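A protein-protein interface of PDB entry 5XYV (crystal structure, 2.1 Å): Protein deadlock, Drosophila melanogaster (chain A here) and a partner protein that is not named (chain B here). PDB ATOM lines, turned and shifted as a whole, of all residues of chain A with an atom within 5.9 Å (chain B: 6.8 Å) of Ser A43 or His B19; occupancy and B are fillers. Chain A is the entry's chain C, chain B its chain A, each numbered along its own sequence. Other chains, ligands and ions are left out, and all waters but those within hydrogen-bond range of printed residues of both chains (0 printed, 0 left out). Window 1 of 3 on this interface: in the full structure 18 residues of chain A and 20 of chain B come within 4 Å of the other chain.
Lys A38 touches none of the printed residues of chain B. Of the printed residues of chain B, Gly A39 touches Tyr B21 (3.3 Å). Of the printed residues of chain B, Phe A40 touches Tyr B21 (3.2 Å) and Phe B30 (3.5 Å). Of the printed residues of chain B, Ser A43 touches His B19 and Tyr B21. Printed residues of chain B within 4 Å of Tyr A48: Leu B18, His B19 and Tyr B58. His B19 touches four residues of chain A. Printed residues of chain A within 4 Å of Tyr B21: Gly A39, Phe A40 and Ser A43. Of the printed residues of chain A, Tyr B58 touches Tyr A48. The nearest residue of chain A that does not touch His B19 is Phe A40 (5.4 Å).
A ring nitrogen (NE2) of His B19 sits at hydrogen-bond distance from the side-chain hydroxyl (OG) of Ser A43, 3.0 Å away. OH of Tyr B21 is in hydrogen-bond range of N of Phe A40 (3.2 Å).
CD2 of Leu A4 touches O of Leu B18, at 3.6 Å. Leu A4 touches His B19. Tyr B21 touches Gly A39 (CE1 to O, 3.3 Å). Phe A40 touches Phe B30 (CE1 to CZ, 3.5 Å). Tyr B21 touches Ser A43 (CD1 to CB, 3.7 Å). Trp A44 touches His B19. Phe B30 touches Trp A44 (CG to CH2, 3.7 Å). OH of Tyr A48 touches O of Leu B18 (3.9 Å). His B19 touches Tyr A48 (ND1 to CE2, 3.3 Å). Tyr B58 touches Tyr A48.
Of the 12 printed residues of chain A, 6 touch a printed residue of chain B. Hydrophobic or aromatic side chains of chain A within 4 Å of the printed part of chain B: Leu A4, Phe A40, Trp A44 and Tyr A48. Among the printed residues, 12 pairs touch across the chains.
N of Leu B18 is in hydrogen-bond range of O of Phe B30 (2.7 Å). The backbone carbonyl oxygen (O) of His B19 lies within hydrogen-bond range of the backbone NH (N) of Phe B30 (2.8 Å). SG of Cys B20 is in hydrogen-bond range of OH of Tyr B58 (3.2 Å). N of Tyr B21 is in hydrogen-bond range of O of Phe B28 (2.8 Å). The backbone carbonyl oxygen (O) of Phe A40 sits at hydrogen-bond distance from the side-chain hydroxyl (OG) of Ser A43. The backbone carbonyl oxygen of Phe A40 sits close to the indole nitrogen of Trp A44.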
ATOM      1  N   LEU A   4      21.212   6.582 -27.952  1.00  0.00           N
ATOM      2  CA  LEU A   4      21.242   6.256 -26.529  1.00  0.00           C
ATOM      3  C   LEU A   4      20.429   5.004 -26.180  1.00  0.00           C
ATOM      4  O   LEU A   4      20.608   4.437 -25.109  1.00  0.00           O
ATOM      5  CB  LEU A   4      20.727   7.439 -25.707  1.00  0.00           C
ATOM      6  CG  LEU A   4      21.481   8.759 -25.885  1.00  0.00           C
ATOM      7  CD1 LEU A   4      20.955   9.802 -24.930  1.00  0.00           C
ATOM      8  CD2 LEU A   4      22.970   8.575 -25.718  1.00  0.00           C
ATOM      9  N   LYS A  38      16.729   9.722 -10.129  1.00  0.00           N
ATOM     10  CA  LYS A  38      15.516   9.597 -10.931  1.00  0.00           C
ATOM     11  C   LYS A  38      15.587  10.433 -12.212  1.00  0.00           C
ATOM     12  O   LYS A  38      15.122  10.013 -13.265  1.00  0.00           O
ATOM     13  CB  LYS A  38      14.292  10.001 -10.109  1.00  0.00           C
ATOM     14  CG  LYS A  38      12.963   9.826 -10.841  1.00  0.00           C
ATOM     15  CD  LYS A  38      11.807  10.158  -9.912  1.00  0.00           C
ATOM     16  CE  LYS A  38      10.457   9.974 -10.575  1.00  0.00           C
ATOM     17  NZ  LYS A  38       9.391  10.334  -9.600  1.00  0.00           N
ATOM     18  N   GLY A  39      16.167  11.619 -12.118  1.00  0.00           N
ATOM     19  CA  GLY A  39      16.366  12.443 -13.292  1.00  0.00           C
ATOM     20  C   GLY A  39      17.517  11.936 -14.155  1.00  0.00           C
ATOM     21  O   GLY A  39      17.550  12.166 -15.361  1.00  0.00           O
ATOM     22  N   PHE A  40      18.470  11.246 -13.539  1.00  0.00           N
ATOM     23  CA  PHE A  40      19.564  10.636 -14.300  1.00  0.00           C
ATOM     24  C   PHE A  40      19.047   9.552 -15.229  1.00  0.00           C
ATOM     25  O   PHE A  40      19.484   9.441 -16.359  1.00  0.00           O
ATOM     26  CB  PHE A  40      20.606  10.071 -13.339  1.00  0.00           C
ATOM     27  CG  PHE A  40      21.584   9.128 -13.977  1.00  0.00           C
ATOM     28  CD1 PHE A  40      22.617   9.611 -14.789  1.00  0.00           C
ATOM     29  CD2 PHE A  40      21.498   7.767 -13.746  1.00  0.00           C
ATOM     30  CE1 PHE A  40      23.536   8.728 -15.373  1.00  0.00           C
ATOM     31  CE2 PHE A  40      22.434   6.888 -14.301  1.00  0.00           C
ATOM     32  CZ  PHE A  40      23.444   7.376 -15.126  1.00  0.00           C
ATOM     33  N   LEU A  41      18.116   8.742 -14.754  1.00  0.00           N
ATOM     34  CA  LEU A  41      17.576   7.669 -15.577  1.00  0.00           C
ATOM     35  C   LEU A  41      16.659   8.193 -16.678  1.00  0.00           C
ATOM     36  O   LEU A  41      16.699   7.716 -17.816  1.00  0.00           O
ATOM     37  CB  LEU A  41      16.829   6.660 -14.716  1.00  0.00           C
ATOM     38  CG  LEU A  41      17.722   5.788 -13.838  1.00  0.00           C
ATOM     39  CD1 LEU A  41      16.851   4.902 -12.989  1.00  0.00           C
ATOM     40  CD2 LEU A  41      18.683   4.966 -14.687  1.00  0.00           C
ATOM     41  N   GLU A  42      15.863   9.199 -16.330  1.00  0.00           N
ATOM     42  CA  GLU A  42      14.995   9.873 -17.278  1.00  0.00           C
ATOM     43  C   GLU A  42      15.785  10.614 -18.374  1.00  0.00           C
ATOM     44  O   GLU A  42      15.259  10.830 -19.461  1.00  0.00           O
ATOM     45  CB  GLU A  42      14.051  10.845 -16.530  1.00  0.00           C
ATOM     46  CG  GLU A  42      13.037  10.137 -15.618  1.00  0.00           C
ATOM     47  CD  GLU A  42      12.265  11.072 -14.688  1.00  0.00           C
ATOM     48  OE1 GLU A  42      12.550  12.289 -14.669  1.00  0.00           O
ATOM     49  OE2 GLU A  42      11.405  10.569 -13.929  1.00  0.00           O
ATOM     50  N   SER A  43      17.036  10.993 -18.093  1.00  0.00           N
ATOM     51  CA  SER A  43      17.816  11.813 -19.023  1.00  0.00           C
ATOM     52  C   SER A  43      18.278  11.032 -20.249  1.00  0.00           C
ATOM     53  O   SER A  43      18.516  11.605 -21.313  1.00  0.00           O
ATOM     54  CB  SER A  43      19.035  12.427 -18.330  1.00  0.00           C
ATOM     55  OG  SER A  43      20.111  11.505 -18.294  1.00  0.00           O
ATOM     56  N   TRP A  44      18.420   9.725 -20.100  1.00  0.00           N
ATOM     57  CA  TRP A  44      18.784   8.878 -21.228  1.00  0.00           C
ATOM     58  C   TRP A  44      17.633   8.642 -22.183  1.00  0.00           C
ATOM     59  O   TRP A  44      17.854   8.459 -23.377  1.00  0.00           O
ATOM     60  CB  TRP A  44      19.304   7.520 -20.757  1.00  0.00           C
ATOM     61  CG  TRP A  44      20.477   7.608 -19.869  1.00  0.00           C
ATOM     62  CD1 TRP A  44      20.480   7.743 -18.508  1.00  0.00           C
ATOM     63  CD2 TRP A  44      21.844   7.583 -20.276  1.00  0.00           C
ATOM     64  NE1 TRP A  44      21.774   7.805 -18.051  1.00  0.00           N
ATOM     65  CE2 TRP A  44      22.634   7.704 -19.122  1.00  0.00           C
ATOM     66  CE3 TRP A  44      22.483   7.469 -21.520  1.00  0.00           C
ATOM     67  CZ2 TRP A  44      24.032   7.705 -19.158  1.00  0.00           C
ATOM     68  CZ3 TRP A  44      23.855   7.480 -21.556  1.00  0.00           C
ATOM     69  CH2 TRP A  44      24.619   7.588 -20.382  1.00  0.00           C
ATOM     70  N   ARG A  45      16.411   8.618 -21.655  1.00  0.00           N
ATOM     71  CA  ARG A  45      15.257   8.164 -22.442  1.00  0.00           C
ATOM     72  C   ARG A  45      14.601   9.250 -23.305  1.00  0.00           C
ATOM     73  O   ARG A  45      14.101   8.961 -24.391  1.00  0.00           O
ATOM     74  CB  ARG A  45      14.186   7.522 -21.534  1.00  0.00           C
ATOM     75  CG  ARG A  45      14.706   6.738 -20.335  1.00  0.00           C
ATOM     76  CD  ARG A  45      13.570   5.976 -19.638  1.00  0.00           C
ATOM     77  NE  ARG A  45      12.252   6.555 -19.895  1.00  0.00           N
ATOM     78  CZ  ARG A  45      11.761   7.611 -19.254  1.00  0.00           C
ATOM     79  NH1 ARG A  45      12.476   8.200 -18.306  1.00  0.00           N
ATOM     80  NH2 ARG A  45      10.555   8.070 -19.554  1.00  0.00           N
ATOM     81  N   LYS A  46      14.584  10.487 -22.833  1.00  0.00           N
ATOM     82  CA  LYS A  46      13.923  11.528 -23.596  1.00  0.00           C
ATOM     83  C   LYS A  46      14.913  12.590 -24.070  1.00  0.00           C
ATOM     84  O   LYS A  46      15.860  12.917 -23.355  1.00  0.00           O
ATOM     85  CB  LYS A  46      12.797  12.157 -22.766  1.00  0.00           C
ATOM     86  CG  LYS A  46      11.771  11.162 -22.246  1.00  0.00           C
ATOM     87  CD  LYS A  46      10.369  11.761 -22.252  1.00  0.00           C
ATOM     88  CE  LYS A  46       9.615  11.456 -20.963  1.00  0.00           C
ATOM     89  NZ  LYS A  46       9.075  12.716 -20.375  1.00  0.00           N
ATOM     90  N   PRO A  47      14.684  13.141 -25.279  1.00  0.00           N
ATOM     91  CA  PRO A  47      15.610  14.088 -25.922  1.00  0.00           C
ATOM     92  C   PRO A  47      15.804  15.368 -25.108  1.00  0.00           C
ATOM     93  O   PRO A  47      14.868  15.825 -24.441  1.00  0.00           O
ATOM     94  CB  PRO A  47      14.932  14.400 -27.266  1.00  0.00           C
ATOM     95  CG  PRO A  47      13.829  13.383 -27.407  1.00  0.00           C
ATOM     96  CD  PRO A  47      13.431  13.009 -26.038  1.00  0.00           C
ATOM     97  N   TYR A  48      17.007  15.933 -25.141  1.00  0.00           N
ATOM     98  CA  TYR A  48      17.280  17.118 -24.335  1.00  0.00           C
ATOM     99  C   TYR A  48      17.106  18.427 -25.095  1.00  0.00           C
ATOM    100  O   TYR A  48      17.297  18.499 -26.303  1.00  0.00           O
ATOM    101  CB  TYR A  48      18.691  17.054 -23.739  1.00  0.00           C
ATOM    102  CG  TYR A  48      19.655  16.171 -24.494  1.00  0.00           C
ATOM    103  CD1 TYR A  48      20.376  16.659 -25.571  1.00  0.00           C
ATOM    104  CD2 TYR A  48      19.875  14.855 -24.099  1.00  0.00           C
ATOM    105  CE1 TYR A  48      21.244  15.850 -26.256  1.00  0.00           C
ATOM    106  CE2 TYR A  48      20.763  14.042 -24.776  1.00  0.00           C
ATOM    107  CZ  TYR A  48      21.451  14.550 -25.852  1.00  0.00           C
ATOM    108  OH  TYR A  48      22.339  13.739 -26.521  1.00  0.00           O
ATOM    109  N   LYS B  16      34.278   9.387 -28.138  1.00  0.00           N
ATOM    110  CA  LYS B  16      33.051  10.114 -28.412  1.00  0.00           C
ATOM    111  C   LYS B  16      32.368  10.583 -27.137  1.00  0.00           C
ATOM    112  O   LYS B  16      32.447   9.925 -26.093  1.00  0.00           O
ATOM    113  CB  LYS B  16      32.088   9.234 -29.218  1.00  0.00           C
ATOM    114  CG  LYS B  16      31.058  10.008 -30.036  1.00  0.00           C
ATOM    115  CD  LYS B  16      30.121   9.068 -30.808  1.00  0.00           C
ATOM    116  CE  LYS B  16      28.802   9.768 -31.163  1.00  0.00           C
ATOM    117  NZ  LYS B  16      27.748   8.849 -31.703  1.00  0.00           N
ATOM    118  N   ILE B  17      31.718  11.734 -27.232  1.00  0.00           N
ATOM    119  CA  ILE B  17      30.869  12.237 -26.169  1.00  0.00           C
ATOM    120  C   ILE B  17      29.436  11.833 -26.461  1.00  0.00           C
ATOM    121  O   ILE B  17      28.868  12.274 -27.449  1.00  0.00           O
ATOM    122  CB  ILE B  17      30.951  13.763 -26.026  1.00  0.00           C
ATOM    123  CG1 ILE B  17      32.377  14.165 -25.656  1.00  0.00           C
ATOM    124  CG2 ILE B  17      29.911  14.241 -24.999  1.00  0.00           C
ATOM    125  CD1 ILE B  17      32.589  15.626 -25.426  1.00  0.00           C
ATOM    126  N   LEU B  18      28.846  11.001 -25.605  1.00  0.00           N
ATOM    127  CA  LEU B  18      27.558  10.406 -25.953  1.00  0.00           C
ATOM    128  C   LEU B  18      26.383  11.190 -25.386  1.00  0.00           C
ATOM    129  O   LEU B  18      25.308  11.238 -25.987  1.00  0.00           O
ATOM    130  CB  LEU B  18      27.489   8.954 -25.481  1.00  0.00           C
ATOM    131  CG  LEU B  18      28.443   7.994 -26.207  1.00  0.00           C
ATOM    132  CD1 LEU B  18      28.505   6.612 -25.537  1.00  0.00           C
ATOM    133  CD2 LEU B  18      28.034   7.839 -27.650  1.00  0.00           C
ATOM    134  N   HIS B  19      26.607  11.816 -24.236  1.00  0.00           N
ATOM    135  CA  HIS B  19      25.517  12.285 -23.405  1.00  0.00           C
ATOM    136  C   HIS B  19      26.081  13.134 -22.284  1.00  0.00           C
ATOM    137  O   HIS B  19      27.291  13.151 -22.043  1.00  0.00           O
ATOM    138  CB  HIS B  19      24.731  11.090 -22.843  1.00  0.00           C
ATOM    139  CG  HIS B  19      23.470  11.454 -22.115  1.00  0.00           C
ATOM    140  ND1 HIS B  19      22.522  12.322 -22.637  1.00  0.00           N
ATOM    141  CD2 HIS B  19      22.972  11.043 -20.929  1.00  0.00           C
ATOM    142  CE1 HIS B  19      21.522  12.435 -21.794  1.00  0.00           C
ATOM    143  NE2 HIS B  19      21.761  11.665 -20.745  1.00  0.00           N
ATOM    144  N   CYS B  20      25.198  13.845 -21.604  1.00  0.00           N
ATOM    145  CA  CYS B  20      25.567  14.619 -20.439  1.00  0.00           C
ATOM    146  C   CYS B  20      24.415  14.659 -19.447  1.00  0.00           C
ATOM    147  O   CYS B  20      23.261  14.434 -19.802  1.00  0.00           O
ATOM    148  CB  CYS B  20      25.982  16.038 -20.836  1.00  0.00           C
ATOM    149  SG  CYS B  20      24.617  17.118 -21.367  1.00  0.00           S
ATOM    150  N   TYR B  21      24.738  14.930 -18.192  1.00  0.00           N
ATOM    151  CA  TYR B  21      23.711  15.095 -17.181  1.00  0.00           C
ATOM    152  C   TYR B  21      24.167  16.192 -16.239  1.00  0.00           C
ATOM    153  O   TYR B  21      25.333  16.250 -15.844  1.00  0.00           O
ATOM    154  CB  TYR B  21      23.446  13.781 -16.456  1.00  0.00           C
ATOM    155  CG  TYR B  21      22.362  13.868 -15.418  1.00  0.00           C
ATOM    156  CD1 TYR B  21      21.045  14.142 -15.769  1.00  0.00           C
ATOM    157  CD2 TYR B  21      22.656  13.682 -14.086  1.00  0.00           C
ATOM    158  CE1 TYR B  21      20.058  14.219 -14.802  1.00  0.00           C
ATOM    159  CE2 TYR B  21      21.692  13.759 -13.129  1.00  0.00           C
ATOM    160  CZ  TYR B  21      20.396  14.031 -13.480  1.00  0.00           C
ATOM    161  OH  TYR B  21      19.441  14.093 -12.485  1.00  0.00           O
ATOM    162  N   GLN B  22      23.239  17.076 -15.896  1.00  0.00           N
ATOM    163  CA  GLN B  22      23.544  18.241 -15.084  1.00  0.00           C
ATOM    164  C   GLN B  22      22.929  18.091 -13.706  1.00  0.00           C
ATOM    165  O   GLN B  22      21.740  17.824 -13.595  1.00  0.00           O
ATOM    166  CB  GLN B  22      23.013  19.489 -15.781  1.00  0.00           C
ATOM    167  CG  GLN B  22      23.270  20.819 -15.112  1.00  0.00           C
ATOM    168  CD  GLN B  22      22.634  21.946 -15.914  1.00  0.00           C
ATOM    169  OE1 GLN B  22      21.415  21.983 -16.087  1.00  0.00           O
ATOM    170  NE2 GLN B  22      23.462  22.842 -16.441  1.00  0.00           N
ATOM    171  N   PHE B  28      28.219  16.353 -15.874  1.00  0.00           N
ATOM    172  CA  PHE B  28      28.967  15.152 -16.234  1.00  0.00           C
ATOM    173  C   PHE B  28      28.719  14.808 -17.678  1.00  0.00           C
ATOM    174  O   PHE B  28      27.571  14.795 -18.128  1.00  0.00           O
ATOM    175  CB  PHE B  28      28.584  13.953 -15.350  1.00  0.00           C
ATOM    176  CG  PHE B  28      29.114  14.048 -13.943  1.00  0.00           C
ATOM    177  CD1 PHE B  28      30.304  13.421 -13.588  1.00  0.00           C
ATOM    178  CD2 PHE B  28      28.435  14.780 -12.976  1.00  0.00           C
ATOM    179  CE1 PHE B  28      30.799  13.520 -12.297  1.00  0.00           C
ATOM    180  CE2 PHE B  28      28.936  14.880 -11.685  1.00  0.00           C
ATOM    181  CZ  PHE B  28      30.123  14.255 -11.353  1.00  0.00           C
ATOM    182  N   MET B  29      29.807  14.537 -18.389  1.00  0.00           N
ATOM    183  CA  MET B  29      29.757  13.979 -19.722  1.00  0.00           C
ATOM    184  C   MET B  29      29.915  12.462 -19.657  1.00  0.00           C
ATOM    185  O   MET B  29      30.727  11.947 -18.903  1.00  0.00           O
ATOM    186  CB  MET B  29      30.854  14.574 -20.610  1.00  0.00           C
ATOM    187  CG  MET B  29      31.180  16.042 -20.348  1.00  0.00           C
ATOM    188  SD  MET B  29      29.826  17.124 -20.816  1.00  0.00           S
ATOM    189  CE  MET B  29      29.786  16.942 -22.603  1.00  0.00           C
ATOM    190  N   PHE B  30      29.125  11.762 -20.458  1.00  0.00           N
ATOM    191  CA  PHE B  30      29.231  10.327 -20.600  1.00  0.00           C
ATOM    192  C   PHE B  30      29.926  10.047 -21.922  1.00  0.00           C
ATOM    193  O   PHE B  30      29.422  10.425 -22.983  1.00  0.00           O
ATOM    194  CB  PHE B  30      27.843   9.684 -20.510  1.00  0.00           C
ATOM    195  CG  PHE B  30      27.116  10.062 -19.248  1.00  0.00           C
ATOM    196  CD1 PHE B  30      27.471   9.488 -18.036  1.00  0.00           C
ATOM    197  CD2 PHE B  30      26.130  11.044 -19.263  1.00  0.00           C
ATOM    198  CE1 PHE B  30      26.839   9.852 -16.853  1.00  0.00           C
ATOM    199  CE2 PHE B  30      25.480  11.409 -18.090  1.00  0.00           C
ATOM    200  CZ  PHE B  30      25.840  10.810 -16.879  1.00  0.00           C
ATOM    201  N   VAL B  31      31.103   9.429 -21.838  1.00  0.00           N
ATOM    202  CA  VAL B  31      32.014   9.310 -22.979  1.00  0.00           C
ATOM    203  C   VAL B  31      32.553   7.908 -23.219  1.00  0.00           C
ATOM    204  O   VAL B  31      32.503   7.042 -22.341  1.00  0.00           O
ATOM    205  CB  VAL B  31      33.229  10.225 -22.807  1.00  0.00           C
ATOM    206  CG1 VAL B  31      32.781  11.673 -22.541  1.00  0.00           C
ATOM    207  CG2 VAL B  31      34.153   9.695 -21.682  1.00  0.00           C
ATOM    208  N   TYR B  58      29.636  18.696 -29.194  1.00  0.00           N
ATOM    209  CA  TYR B  58      28.531  17.983 -28.558  1.00  0.00           C
ATOM    210  C   TYR B  58      27.358  18.921 -28.206  1.00  0.00           C
ATOM    211  O   TYR B  58      26.203  18.583 -28.447  1.00  0.00           O
ATOM    212  CB  TYR B  58      28.989  17.252 -27.286  1.00  0.00           C
ATOM    213  CG  TYR B  58      27.809  16.806 -26.448  1.00  0.00           C
ATOM    214  CD1 TYR B  58      27.067  15.686 -26.793  1.00  0.00           C
ATOM    215  CD2 TYR B  58      27.423  17.516 -25.339  1.00  0.00           C
ATOM    216  CE1 TYR B  58      25.961  15.289 -26.032  1.00  0.00           C
ATOM    217  CE2 TYR B  58      26.328  17.132 -24.576  1.00  0.00           C
ATOM    218  CZ  TYR B  58      25.608  16.012 -24.931  1.00  0.00           C
ATOM    219  OH  TYR B  58      24.519  15.650 -24.179  1.00  0.00           O
